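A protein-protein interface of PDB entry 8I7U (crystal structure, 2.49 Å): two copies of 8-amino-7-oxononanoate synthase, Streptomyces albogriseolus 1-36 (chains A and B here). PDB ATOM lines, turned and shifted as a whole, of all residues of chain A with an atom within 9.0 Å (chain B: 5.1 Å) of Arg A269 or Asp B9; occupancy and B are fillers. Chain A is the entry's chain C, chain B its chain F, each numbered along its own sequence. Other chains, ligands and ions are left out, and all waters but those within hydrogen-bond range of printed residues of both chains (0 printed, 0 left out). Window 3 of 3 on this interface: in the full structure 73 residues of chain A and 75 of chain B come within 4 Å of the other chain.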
ATOM      1  N   ALA A 113      -8.406   7.314  15.050  1.00  0.00           N
ATOM      2  CA  ALA A 113      -8.224   6.517  13.854  1.00  0.00           C
ATOM      3  C   ALA A 113      -7.332   5.319  14.115  1.00  0.00           C
ATOM      4  O   ALA A 113      -7.457   4.305  13.420  1.00  0.00           O
ATOM      5  CB  ALA A 113      -7.644   7.378  12.729  1.00  0.00           C
ATOM      6  N   VAL A 117      -8.007   0.328  15.828  1.00  0.00           N
ATOM      7  CA  VAL A 117      -7.345  -0.557  14.881  1.00  0.00           C
ATOM      8  C   VAL A 117      -6.246  -1.355  15.569  1.00  0.00           C
ATOM      9  O   VAL A 117      -6.136  -2.574  15.387  1.00  0.00           O
ATOM     10  CB  VAL A 117      -6.785   0.257  13.704  1.00  0.00           C
ATOM     11  CG1 VAL A 117      -6.118  -0.657  12.712  1.00  0.00           C
ATOM     12  CG2 VAL A 117      -7.879   1.080  13.048  1.00  0.00           C
ATOM     13  N   LEU A 122      -5.267  -5.836  13.623  1.00  0.00           N
ATOM     14  CA  LEU A 122      -4.903  -5.689  12.216  1.00  0.00           C
ATOM     15  C   LEU A 122      -3.484  -5.164  12.037  1.00  0.00           C
ATOM     16  O   LEU A 122      -2.881  -5.375  10.980  1.00  0.00           O
ATOM     17  CB  LEU A 122      -5.895  -4.765  11.523  1.00  0.00           C
ATOM     18  CG  LEU A 122      -7.333  -5.272  11.459  1.00  0.00           C
ATOM     19  CD1 LEU A 122      -8.292  -4.099  11.423  1.00  0.00           C
ATOM     20  CD2 LEU A 122      -7.522  -6.113  10.225  1.00  0.00           C
ATOM     21  N   PHE A 255       3.206   6.134  10.890  1.00  0.00           N
ATOM     22  CA  PHE A 255       2.763   4.736  10.846  1.00  0.00           C
ATOM     23  C   PHE A 255       3.867   3.739  11.178  1.00  0.00           C
ATOM     24  O   PHE A 255       3.587   2.679  11.746  1.00  0.00           O
ATOM     25  CB  PHE A 255       2.215   4.390   9.471  1.00  0.00           C
ATOM     26  CG  PHE A 255       0.946   5.082   9.128  1.00  0.00           C
ATOM     27  CD1 PHE A 255      -0.228   4.785   9.796  1.00  0.00           C
ATOM     28  CD2 PHE A 255       0.918   6.008   8.108  1.00  0.00           C
ATOM     29  CE1 PHE A 255      -1.407   5.431   9.477  1.00  0.00           C
ATOM     30  CE2 PHE A 255      -0.267   6.653   7.765  1.00  0.00           C
ATOM     31  CZ  PHE A 255      -1.425   6.368   8.460  1.00  0.00           C
ATOM     32  N   ASP A 261       3.735   0.187   3.098  1.00  0.00           N
ATOM     33  CA  ASP A 261       2.422   0.816   3.004  1.00  0.00           C
ATOM     34  C   ASP A 261       1.342   0.091   3.802  1.00  0.00           C
ATOM     35  O   ASP A 261       0.198   0.556   3.828  1.00  0.00           O
ATOM     36  CB  ASP A 261       1.985   0.941   1.534  1.00  0.00           C
ATOM     37  CG  ASP A 261       1.950  -0.404   0.786  1.00  0.00           C
ATOM     38  OD1 ASP A 261       1.946  -1.486   1.419  1.00  0.00           O
ATOM     39  OD2 ASP A 261       1.934  -0.373  -0.464  1.00  0.00           O
ATOM     40  N   ARG A 262       1.670  -1.016   4.465  1.00  0.00           N
ATOM     41  CA  ARG A 262       0.621  -1.872   5.001  1.00  0.00           C
ATOM     42  C   ARG A 262      -0.168  -1.176   6.105  1.00  0.00           C
ATOM     43  O   ARG A 262      -1.407  -1.156   6.067  1.00  0.00           O
ATOM     44  CB  ARG A 262       1.221  -3.192   5.477  1.00  0.00           C
ATOM     45  CG  ARG A 262       1.641  -4.090   4.307  1.00  0.00           C
ATOM     46  CD  ARG A 262       2.362  -5.338   4.770  1.00  0.00           C
ATOM     47  NE  ARG A 262       3.592  -5.006   5.474  1.00  0.00           N
ATOM     48  CZ  ARG A 262       4.340  -5.881   6.130  1.00  0.00           C
ATOM     49  NH1 ARG A 262       4.008  -7.159   6.197  1.00  0.00           N
ATOM     50  NH2 ARG A 262       5.444  -5.461   6.742  1.00  0.00           N
ATOM     51  N   LYS A 263       0.526  -0.576   7.086  1.00  0.00           N
ATOM     52  CA  LYS A 263      -0.172   0.058   8.206  1.00  0.00           C
ATOM     53  C   LYS A 263      -1.051   1.216   7.737  1.00  0.00           C
ATOM     54  O   LYS A 263      -2.205   1.337   8.162  1.00  0.00           O
ATOM     55  CB  LYS A 263       0.831   0.535   9.254  1.00  0.00           C
ATOM     56  CG  LYS A 263       1.605  -0.591   9.931  1.00  0.00           C
ATOM     57  CD  LYS A 263       1.927  -0.268  11.383  1.00  0.00           C
ATOM     58  CE  LYS A 263       2.393  -1.502  12.144  1.00  0.00           C
ATOM     59  NZ  LYS A 263       3.701  -1.999  11.629  1.00  0.00           N
ATOM     60  N   ARG A 264      -0.530   2.075   6.857  1.00  0.00           N
ATOM     61  CA  ARG A 264      -1.363   3.120   6.265  1.00  0.00           C
ATOM     62  C   ARG A 264      -2.580   2.529   5.541  1.00  0.00           C
ATOM     63  O   ARG A 264      -3.708   3.003   5.720  1.00  0.00           O
ATOM     64  CB  ARG A 264      -0.537   3.988   5.311  1.00  0.00           C
ATOM     65  CG  ARG A 264      -1.376   5.076   4.650  1.00  0.00           C
ATOM     66  CD  ARG A 264      -0.709   5.665   3.430  1.00  0.00           C
ATOM     67  NE  ARG A 264       0.425   6.514   3.764  1.00  0.00           N
ATOM     68  CZ  ARG A 264       0.354   7.829   3.937  1.00  0.00           C
ATOM     69  NH1 ARG A 264      -0.800   8.473   3.877  1.00  0.00           N
ATOM     70  NH2 ARG A 264       1.472   8.515   4.177  1.00  0.00           N
ATOM     71  N   LYS A 265      -2.373   1.495   4.715  1.00  0.00           N
ATOM     72  CA  LYS A 265      -3.500   0.863   4.020  1.00  0.00           C
ATOM     73  C   LYS A 265      -4.540   0.347   5.008  1.00  0.00           C
ATOM     74  O   LYS A 265      -5.739   0.609   4.859  1.00  0.00           O
ATOM     75  CB  LYS A 265      -3.020  -0.287   3.121  1.00  0.00           C
ATOM     76  CG  LYS A 265      -2.543   0.130   1.733  1.00  0.00           C
ATOM     77  CD  LYS A 265      -2.087  -1.062   0.917  1.00  0.00           C
ATOM     78  CE  LYS A 265      -1.312  -0.613  -0.320  1.00  0.00           C
ATOM     79  NZ  LYS A 265      -0.964  -1.750  -1.216  1.00  0.00           N
ATOM     80  N   ILE A 266      -4.094  -0.392   6.026  1.00  0.00           N
ATOM     81  CA  ILE A 266      -5.019  -0.965   6.998  1.00  0.00           C
ATOM     82  C   ILE A 266      -5.811   0.134   7.693  1.00  0.00           C
ATOM     83  O   ILE A 266      -7.032   0.027   7.878  1.00  0.00           O
ATOM     84  CB  ILE A 266      -4.255  -1.824   8.019  1.00  0.00           C
ATOM     85  CG1 ILE A 266      -3.603  -3.028   7.345  1.00  0.00           C
ATOM     86  CG2 ILE A 266      -5.172  -2.250   9.151  1.00  0.00           C
ATOM     87  CD1 ILE A 266      -2.553  -3.672   8.201  1.00  0.00           C
ATOM     88  N   ILE A 267      -5.127   1.210   8.091  1.00  0.00           N
ATOM     89  CA  ILE A 267      -5.788   2.258   8.856  1.00  0.00           C
ATOM     90  C   ILE A 267      -6.670   3.107   7.952  1.00  0.00           C
ATOM     91  O   ILE A 267      -7.786   3.482   8.330  1.00  0.00           O
ATOM     92  CB  ILE A 267      -4.742   3.092   9.610  1.00  0.00           C
ATOM     93  CG1 ILE A 267      -4.241   2.276  10.800  1.00  0.00           C
ATOM     94  CG2 ILE A 267      -5.342   4.423  10.061  1.00  0.00           C
ATOM     95  CD1 ILE A 267      -2.805   2.544  11.179  1.00  0.00           C
ATOM     96  N   GLN A 268      -6.202   3.407   6.742  1.00  0.00           N
ATOM     97  CA  GLN A 268      -7.041   4.146   5.803  1.00  0.00           C
ATOM     98  C   GLN A 268      -8.305   3.384   5.424  1.00  0.00           C
ATOM     99  O   GLN A 268      -9.328   4.007   5.126  1.00  0.00           O
ATOM    100  CB  GLN A 268      -6.254   4.487   4.541  1.00  0.00           C
ATOM    101  CG  GLN A 268      -5.523   5.780   4.640  1.00  0.00           C
ATOM    102  CD  GLN A 268      -4.582   6.002   3.483  1.00  0.00           C
ATOM    103  OE1 GLN A 268      -4.579   5.231   2.510  1.00  0.00           O
ATOM    104  NE2 GLN A 268      -3.756   7.056   3.581  1.00  0.00           N
ATOM    105  N   ARG A 269      -8.264   2.054   5.406  1.00  0.00           N
ATOM    106  CA  ARG A 269      -9.449   1.288   5.047  1.00  0.00           C
ATOM    107  C   ARG A 269     -10.326   0.947   6.251  1.00  0.00           C
ATOM    108  O   ARG A 269     -11.339   0.264   6.090  1.00  0.00           O
ATOM    109  CB  ARG A 269      -9.050   0.018   4.280  1.00  0.00           C
ATOM    110  CG  ARG A 269      -8.446   0.306   2.891  1.00  0.00           C
ATOM    111  CD  ARG A 269      -7.463  -0.759   2.456  1.00  0.00           C
ATOM    112  NE  ARG A 269      -6.724  -0.360   1.262  1.00  0.00           N
ATOM    113  CZ  ARG A 269      -6.130  -1.207   0.424  1.00  0.00           C
ATOM    114  NH1 ARG A 269      -6.162  -2.516   0.623  1.00  0.00           N
ATOM    115  NH2 ARG A 269      -5.510  -0.732  -0.653  1.00  0.00           N
ATOM    116  N   SER A 270      -9.989   1.433   7.438  1.00  0.00           N
ATOM    117  CA  SER A 270     -10.838   1.245   8.602  1.00  0.00           C
ATOM    118  C   SER A 270     -11.900   2.330   8.674  1.00  0.00           C
ATOM    119  O   SER A 270     -11.807   3.372   8.026  1.00  0.00           O
ATOM    120  CB  SER A 270     -10.014   1.259   9.886  1.00  0.00           C
ATOM    121  OG  SER A 270      -9.044   0.228   9.867  1.00  0.00           O
ATOM    122  N   SER A 271     -12.916   2.081   9.488  1.00  0.00           N
ATOM    123  CA  SER A 271     -13.930   3.097   9.763  1.00  0.00           C
ATOM    124  C   SER A 271     -13.444   3.958  10.920  1.00  0.00           C
ATOM    125  O   SER A 271     -13.665   3.657  12.094  1.00  0.00           O
ATOM    126  CB  SER A 271     -15.279   2.461  10.068  1.00  0.00           C
ATOM    127  OG  SER A 271     -16.144   3.414  10.661  1.00  0.00           O
ATOM    128  N   GLY A 272     -12.772   5.042  10.582  1.00  0.00           N
ATOM    129  CA  GLY A 272     -12.350   6.005  11.567  1.00  0.00           C
ATOM    130  C   GLY A 272     -12.196   7.362  10.928  1.00  0.00           C
ATOM    131  O   GLY A 272     -12.475   7.547   9.735  1.00  0.00           O
ATOM    132  N   LEU A 274      -9.716   8.923   9.824  1.00  0.00           N
ATOM    133  CA  LEU A 274      -8.841   9.020   8.657  1.00  0.00           C
ATOM    134  C   LEU A 274      -9.623   8.793   7.375  1.00  0.00           C
ATOM    135  O   LEU A 274      -9.260   9.318   6.314  1.00  0.00           O
ATOM    136  CB  LEU A 274      -7.676   8.023   8.749  1.00  0.00           C
ATOM    137  CG  LEU A 274      -6.590   8.268   7.697  1.00  0.00           C
ATOM    138  CD1 LEU A 274      -6.054   9.684   7.844  1.00  0.00           C
ATOM    139  CD2 LEU A 274      -5.449   7.261   7.769  1.00  0.00           C
ATOM    140  N   MET A 275     -10.712   8.040   7.457  1.00  0.00           N
ATOM    141  CA  MET A 275     -11.539   7.854   6.279  1.00  0.00           C
ATOM    142  C   MET A 275     -12.599   8.937   6.160  1.00  0.00           C
ATOM    143  O   MET A 275     -12.681   9.593   5.126  1.00  0.00           O
ATOM    144  CB  MET A 275     -12.195   6.473   6.293  1.00  0.00           C
ATOM    145  CG  MET A 275     -13.175   6.259   5.138  1.00  0.00           C
ATOM    146  SD  MET A 275     -13.907   4.615   5.157  1.00  0.00           S
ATOM    147  CE  MET A 275     -12.484   3.573   4.824  1.00  0.00           C
ATOM    148  N   TRP A 276     -13.415   9.149   7.194  1.00  0.00           N
ATOM    149  CA  TRP A 276     -14.606   9.981   7.034  1.00  0.00           C
ATOM    150  C   TRP A 276     -14.530  11.351   7.718  1.00  0.00           C
ATOM    151  O   TRP A 276     -15.557  12.019   7.844  1.00  0.00           O
ATOM    152  CB  TRP A 276     -15.852   9.229   7.506  1.00  0.00           C
ATOM    153  CG  TRP A 276     -15.713   8.333   8.722  1.00  0.00           C
ATOM    154  CD1 TRP A 276     -15.725   6.965   8.734  1.00  0.00           C
ATOM    155  CD2 TRP A 276     -15.609   8.742  10.102  1.00  0.00           C
ATOM    156  NE1 TRP A 276     -15.623   6.495  10.028  1.00  0.00           N
ATOM    157  CE2 TRP A 276     -15.553   7.564  10.884  1.00  0.00           C
ATOM    158  CE3 TRP A 276     -15.560   9.980  10.747  1.00  0.00           C
ATOM    159  CZ2 TRP A 276     -15.441   7.592  12.276  1.00  0.00           C
ATOM    160  CZ3 TRP A 276     -15.448  10.003  12.129  1.00  0.00           C
ATOM    161  CH2 TRP A 276     -15.389   8.814  12.877  1.00  0.00           C
ATOM    162  N   ARG B   5     -13.244  -9.240   4.453  1.00  0.00           N
ATOM    163  CA  ARG B   5     -12.343  -8.098   4.475  1.00  0.00           C
ATOM    164  C   ARG B   5     -11.285  -8.184   3.365  1.00  0.00           C
ATOM    165  O   ARG B   5     -11.035  -7.200   2.666  1.00  0.00           O
ATOM    166  CB  ARG B   5     -11.647  -7.971   5.835  1.00  0.00           C
ATOM    167  CG  ARG B   5     -10.672  -6.791   5.913  1.00  0.00           C
ATOM    168  CD  ARG B   5      -9.897  -6.743   7.239  1.00  0.00           C
ATOM    169  NE  ARG B   5      -9.222  -8.006   7.535  1.00  0.00           N
ATOM    170  CZ  ARG B   5      -8.024  -8.340   7.066  1.00  0.00           C
ATOM    171  NH1 ARG B   5      -7.349  -7.537   6.256  1.00  0.00           N
ATOM    172  NH2 ARG B   5      -7.491  -9.510   7.416  1.00  0.00           N
ATOM    173  N   HIS B   6     -10.671  -9.363   3.196  1.00  0.00           N
ATOM    174  CA  HIS B   6      -9.660  -9.541   2.150  1.00  0.00           C
ATOM    175  C   HIS B   6     -10.232  -9.250   0.767  1.00  0.00           C
ATOM    176  O   HIS B   6      -9.541  -8.693  -0.096  1.00  0.00           O
ATOM    177  CB  HIS B   6      -9.086 -10.962   2.188  1.00  0.00           C
ATOM    178  CG  HIS B   6      -8.552 -11.355   3.528  1.00  0.00           C
ATOM    179  ND1 HIS B   6      -9.359 -11.828   4.541  1.00  0.00           N
ATOM    180  CD2 HIS B   6      -7.291 -11.338   4.023  1.00  0.00           C
ATOM    181  CE1 HIS B   6      -8.617 -12.089   5.603  1.00  0.00           C
ATOM    182  NE2 HIS B   6      -7.360 -11.799   5.316  1.00  0.00           N
ATOM    183  N   LEU B   7     -11.486  -9.649   0.530  1.00  0.00           N
ATOM    184  CA  LEU B   7     -12.168  -9.277  -0.707  1.00  0.00           C
ATOM    185  C   LEU B   7     -12.367  -7.769  -0.782  1.00  0.00           C
ATOM    186  O   LEU B   7     -12.141  -7.156  -1.835  1.00  0.00           O
ATOM    187  CB  LEU B   7     -13.516 -10.007  -0.818  1.00  0.00           C
ATOM    188  CG  LEU B   7     -13.486 -11.521  -1.050  1.00  0.00           C
ATOM    189  CD1 LEU B   7     -12.573 -11.831  -2.236  1.00  0.00           C
ATOM    190  CD2 LEU B   7     -13.062 -12.329   0.206  1.00  0.00           C
ATOM    191  N   SER B   8     -12.776  -7.158   0.335  1.00  0.00           N
ATOM    192  CA  SER B   8     -12.918  -5.708   0.382  1.00  0.00           C
ATOM    193  C   SER B   8     -11.584  -5.039   0.085  1.00  0.00           C
ATOM    194  O   SER B   8     -11.497  -4.168  -0.789  1.00  0.00           O
ATOM    195  CB  SER B   8     -13.485  -5.249   1.735  1.00  0.00           C
ATOM    196  OG  SER B   8     -12.514  -5.188   2.763  1.00  0.00           O
ATOM    197  N   ASP B   9     -10.516  -5.482   0.756  1.00  0.00           N
ATOM    198  CA  ASP B   9      -9.187  -4.954   0.453  1.00  0.00           C
ATOM    199  C   ASP B   9      -8.806  -5.271  -0.996  1.00  0.00           C
ATOM    200  O   ASP B   9      -8.210  -4.439  -1.693  1.00  0.00           O
ATOM    201  CB  ASP B   9      -8.136  -5.506   1.443  1.00  0.00           C
ATOM    202  CG  ASP B   9      -8.512  -5.300   2.925  1.00  0.00           C
ATOM    203  OD1 ASP B   9      -9.376  -4.447   3.241  1.00  0.00           O
ATOM    204  OD2 ASP B   9      -7.921  -6.018   3.775  1.00  0.00           O
ATOM    205  N   GLY B  10      -9.184  -6.454  -1.482  1.00  0.00           N
ATOM    206  CA  GLY B  10      -9.014  -6.753  -2.899  1.00  0.00           C
ATOM    207  C   GLY B  10      -9.761  -5.779  -3.793  1.00  0.00           C
ATOM    208  O   GLY B  10      -9.264  -5.386  -4.855  1.00  0.00           O
ATOM    209  N   TYR B  11     -10.955  -5.356  -3.360  1.00  0.00           N
ATOM    210  CA  TYR B  11     -11.683  -4.312  -4.079  1.00  0.00           C
ATOM    211  C   TYR B  11     -10.973  -2.965  -3.969  1.00  0.00           C
ATOM    212  O   TYR B  11     -10.935  -2.207  -4.947  1.00  0.00           O
ATOM    213  CB  TYR B  11     -13.128  -4.196  -3.569  1.00  0.00           C
ATOM    214  CG  TYR B  11     -14.003  -5.382  -3.892  1.00  0.00           C
ATOM    215  CD1 TYR B  11     -13.926  -6.016  -5.133  1.00  0.00           C
ATOM    216  CD2 TYR B  11     -14.899  -5.876  -2.955  1.00  0.00           C
ATOM    217  CE1 TYR B  11     -14.720  -7.108  -5.423  1.00  0.00           C
ATOM    218  CE2 TYR B  11     -15.693  -6.963  -3.233  1.00  0.00           C
ATOM    219  CZ  TYR B  11     -15.599  -7.577  -4.473  1.00  0.00           C
ATOM    220  OH  TYR B  11     -16.390  -8.672  -4.753  1.00  0.00           O
ATOM    221  N   TRP B  12     -10.409  -2.642  -2.786  1.00  0.00           N
ATOM    222  CA  TRP B  12      -9.660  -1.390  -2.650  1.00  0.00           C
ATOM    223  C   TRP B  12      -8.512  -1.332  -3.660  1.00  0.00           C
ATOM    224  O   TRP B  12      -8.279  -0.293  -4.286  1.00  0.00           O
ATOM    225  CB  TRP B  12      -9.101  -1.198  -1.223  1.00  0.00           C
ATOM    226  CG  TRP B  12     -10.082  -0.929  -0.083  1.00  0.00           C
ATOM    227  CD1 TRP B  12     -10.401  -1.794   0.918  1.00  0.00           C
ATOM    228  CD2 TRP B  12     -10.827   0.278   0.185  1.00  0.00           C
ATOM    229  NE1 TRP B  12     -11.309  -1.225   1.771  1.00  0.00           N
ATOM    230  CE2 TRP B  12     -11.588   0.045   1.345  1.00  0.00           C
ATOM    231  CE3 TRP B  12     -10.943   1.511  -0.455  1.00  0.00           C
ATOM    232  CZ2 TRP B  12     -12.449   1.004   1.888  1.00  0.00           C
ATOM    233  CZ3 TRP B  12     -11.808   2.464   0.085  1.00  0.00           C
ATOM    234  CH2 TRP B  12     -12.544   2.204   1.246  1.00  0.00           C
ATOM    235  N   ASP B  13      -7.790  -2.444  -3.838  1.00  0.00           N
ATOM    236  CA  ASP B  13      -6.596  -2.437  -4.683  1.00  0.00           C
ATOM    237  C   ASP B  13      -6.950  -2.131  -6.128  1.00  0.00           C
ATOM    238  O   ASP B  13      -6.311  -1.295  -6.781  1.00  0.00           O
ATOM    239  CB  ASP B  13      -5.871  -3.781  -4.586  1.00  0.00           C
ATOM    240  CG  ASP B  13      -5.096  -3.940  -3.293  1.00  0.00           C
ATOM    241  OD1 ASP B  13      -4.798  -2.914  -2.631  1.00  0.00           O
ATOM    242  OD2 ASP B  13      -4.787  -5.104  -2.945  1.00  0.00           O
ATOM    243  N   PRO B 360     -16.068  -2.712   1.545  1.00  0.00           N
ATOM    244  CA  PRO B 360     -16.986  -2.672   2.684  1.00  0.00           C
ATOM    245  C   PRO B 360     -17.754  -1.364   2.868  1.00  0.00           C
ATOM    246  O   PRO B 360     -18.563  -1.301   3.781  1.00  0.00           O
ATOM    247  CB  PRO B 360     -16.039  -2.888   3.860  1.00  0.00           C
ATOM    248  CG  PRO B 360     -14.769  -2.144   3.430  1.00  0.00           C
ATOM    249  CD  PRO B 360     -14.767  -2.117   1.898  1.00  0.00           C
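The side-chain carboxylate (OD1) of Asp B13 is in salt-bridge range of the guanidinium group (NH2) of Arg A269 (3.0 Å).
Among the printed residues, merely in contact across the chains: Leu A122 with Arg B5, Arg A269 with Asp B9, Arg A269 with Trp B12 and Met A275 with Trp B12.
Printed residues of chain B within 4 Å of Leu A122: Arg B5 (3.7 Å).
Arg A269 touches three residues of chain B.
Of the printed residues of chain B, Met A275 touches Trp B12 (3.8 Å).
Printed residues of chain A within 4 Å of Arg B5: Leu A122.
No residue of chain A comes within 4 Å of Ser B8.
Asp B9 touches just one residue of chain A: Arg A269 (3.6 Å).
No residue of chain A comes within 4 Å of Gly B10.
Tyr B11 touches none of the printed residues of chain A.
The nearest printed residue of chain A that does not touch Asp B13 is Lys A265 (4.2 Å).
Of the 10 printed residues of chain B, 4 touch a printed residue of chain A.
Printed residues of chain B that touch a printed residue of chain A: Arg B5, Asp B9, Trp B12 and Asp B13.
Hydrophobic or aromatic side chains of chain B that line the printed part of chain A: Trp B12.
Along chain B the printed residues that touch a printed residue of chain A span positions 5 to 13.
Hydrophobic or aromatic side chains of chain A within 4 Å of the printed part of chain B: Leu A122 and Met A275.
Among the printed residues, Asp or Glu carboxylates within 4 Å of a Lys or Arg side-chain nitrogen of the other chain: Arg A269 with Asp B13 (3.0 Å).
A ring nitrogen (NE2) of His B6 is in hydrogen-bond range of the guanidinium group of Arg B5 (3.1 Å).
The backbone carbonyl oxygen of Arg B5 is in hydrogen-bond range of the side-chain hydroxyl of Ser B8.
The side-chain carboxylate (OD2) of Asp B9 lies within salt-bridge range of the guanidinium group (NH1) of Arg B5 (3.0 Å).
The side-chain hydroxyl (OG) of Ser B8 sits at hydrogen-bond distance from the side-chain carboxylate (OD1) of Asp B9 (3.3 Å).
No position is printed for both chains.
Of the 5 pairs that touch across the chains among the printed residues, none has its exchanged pair printed and touching as well.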
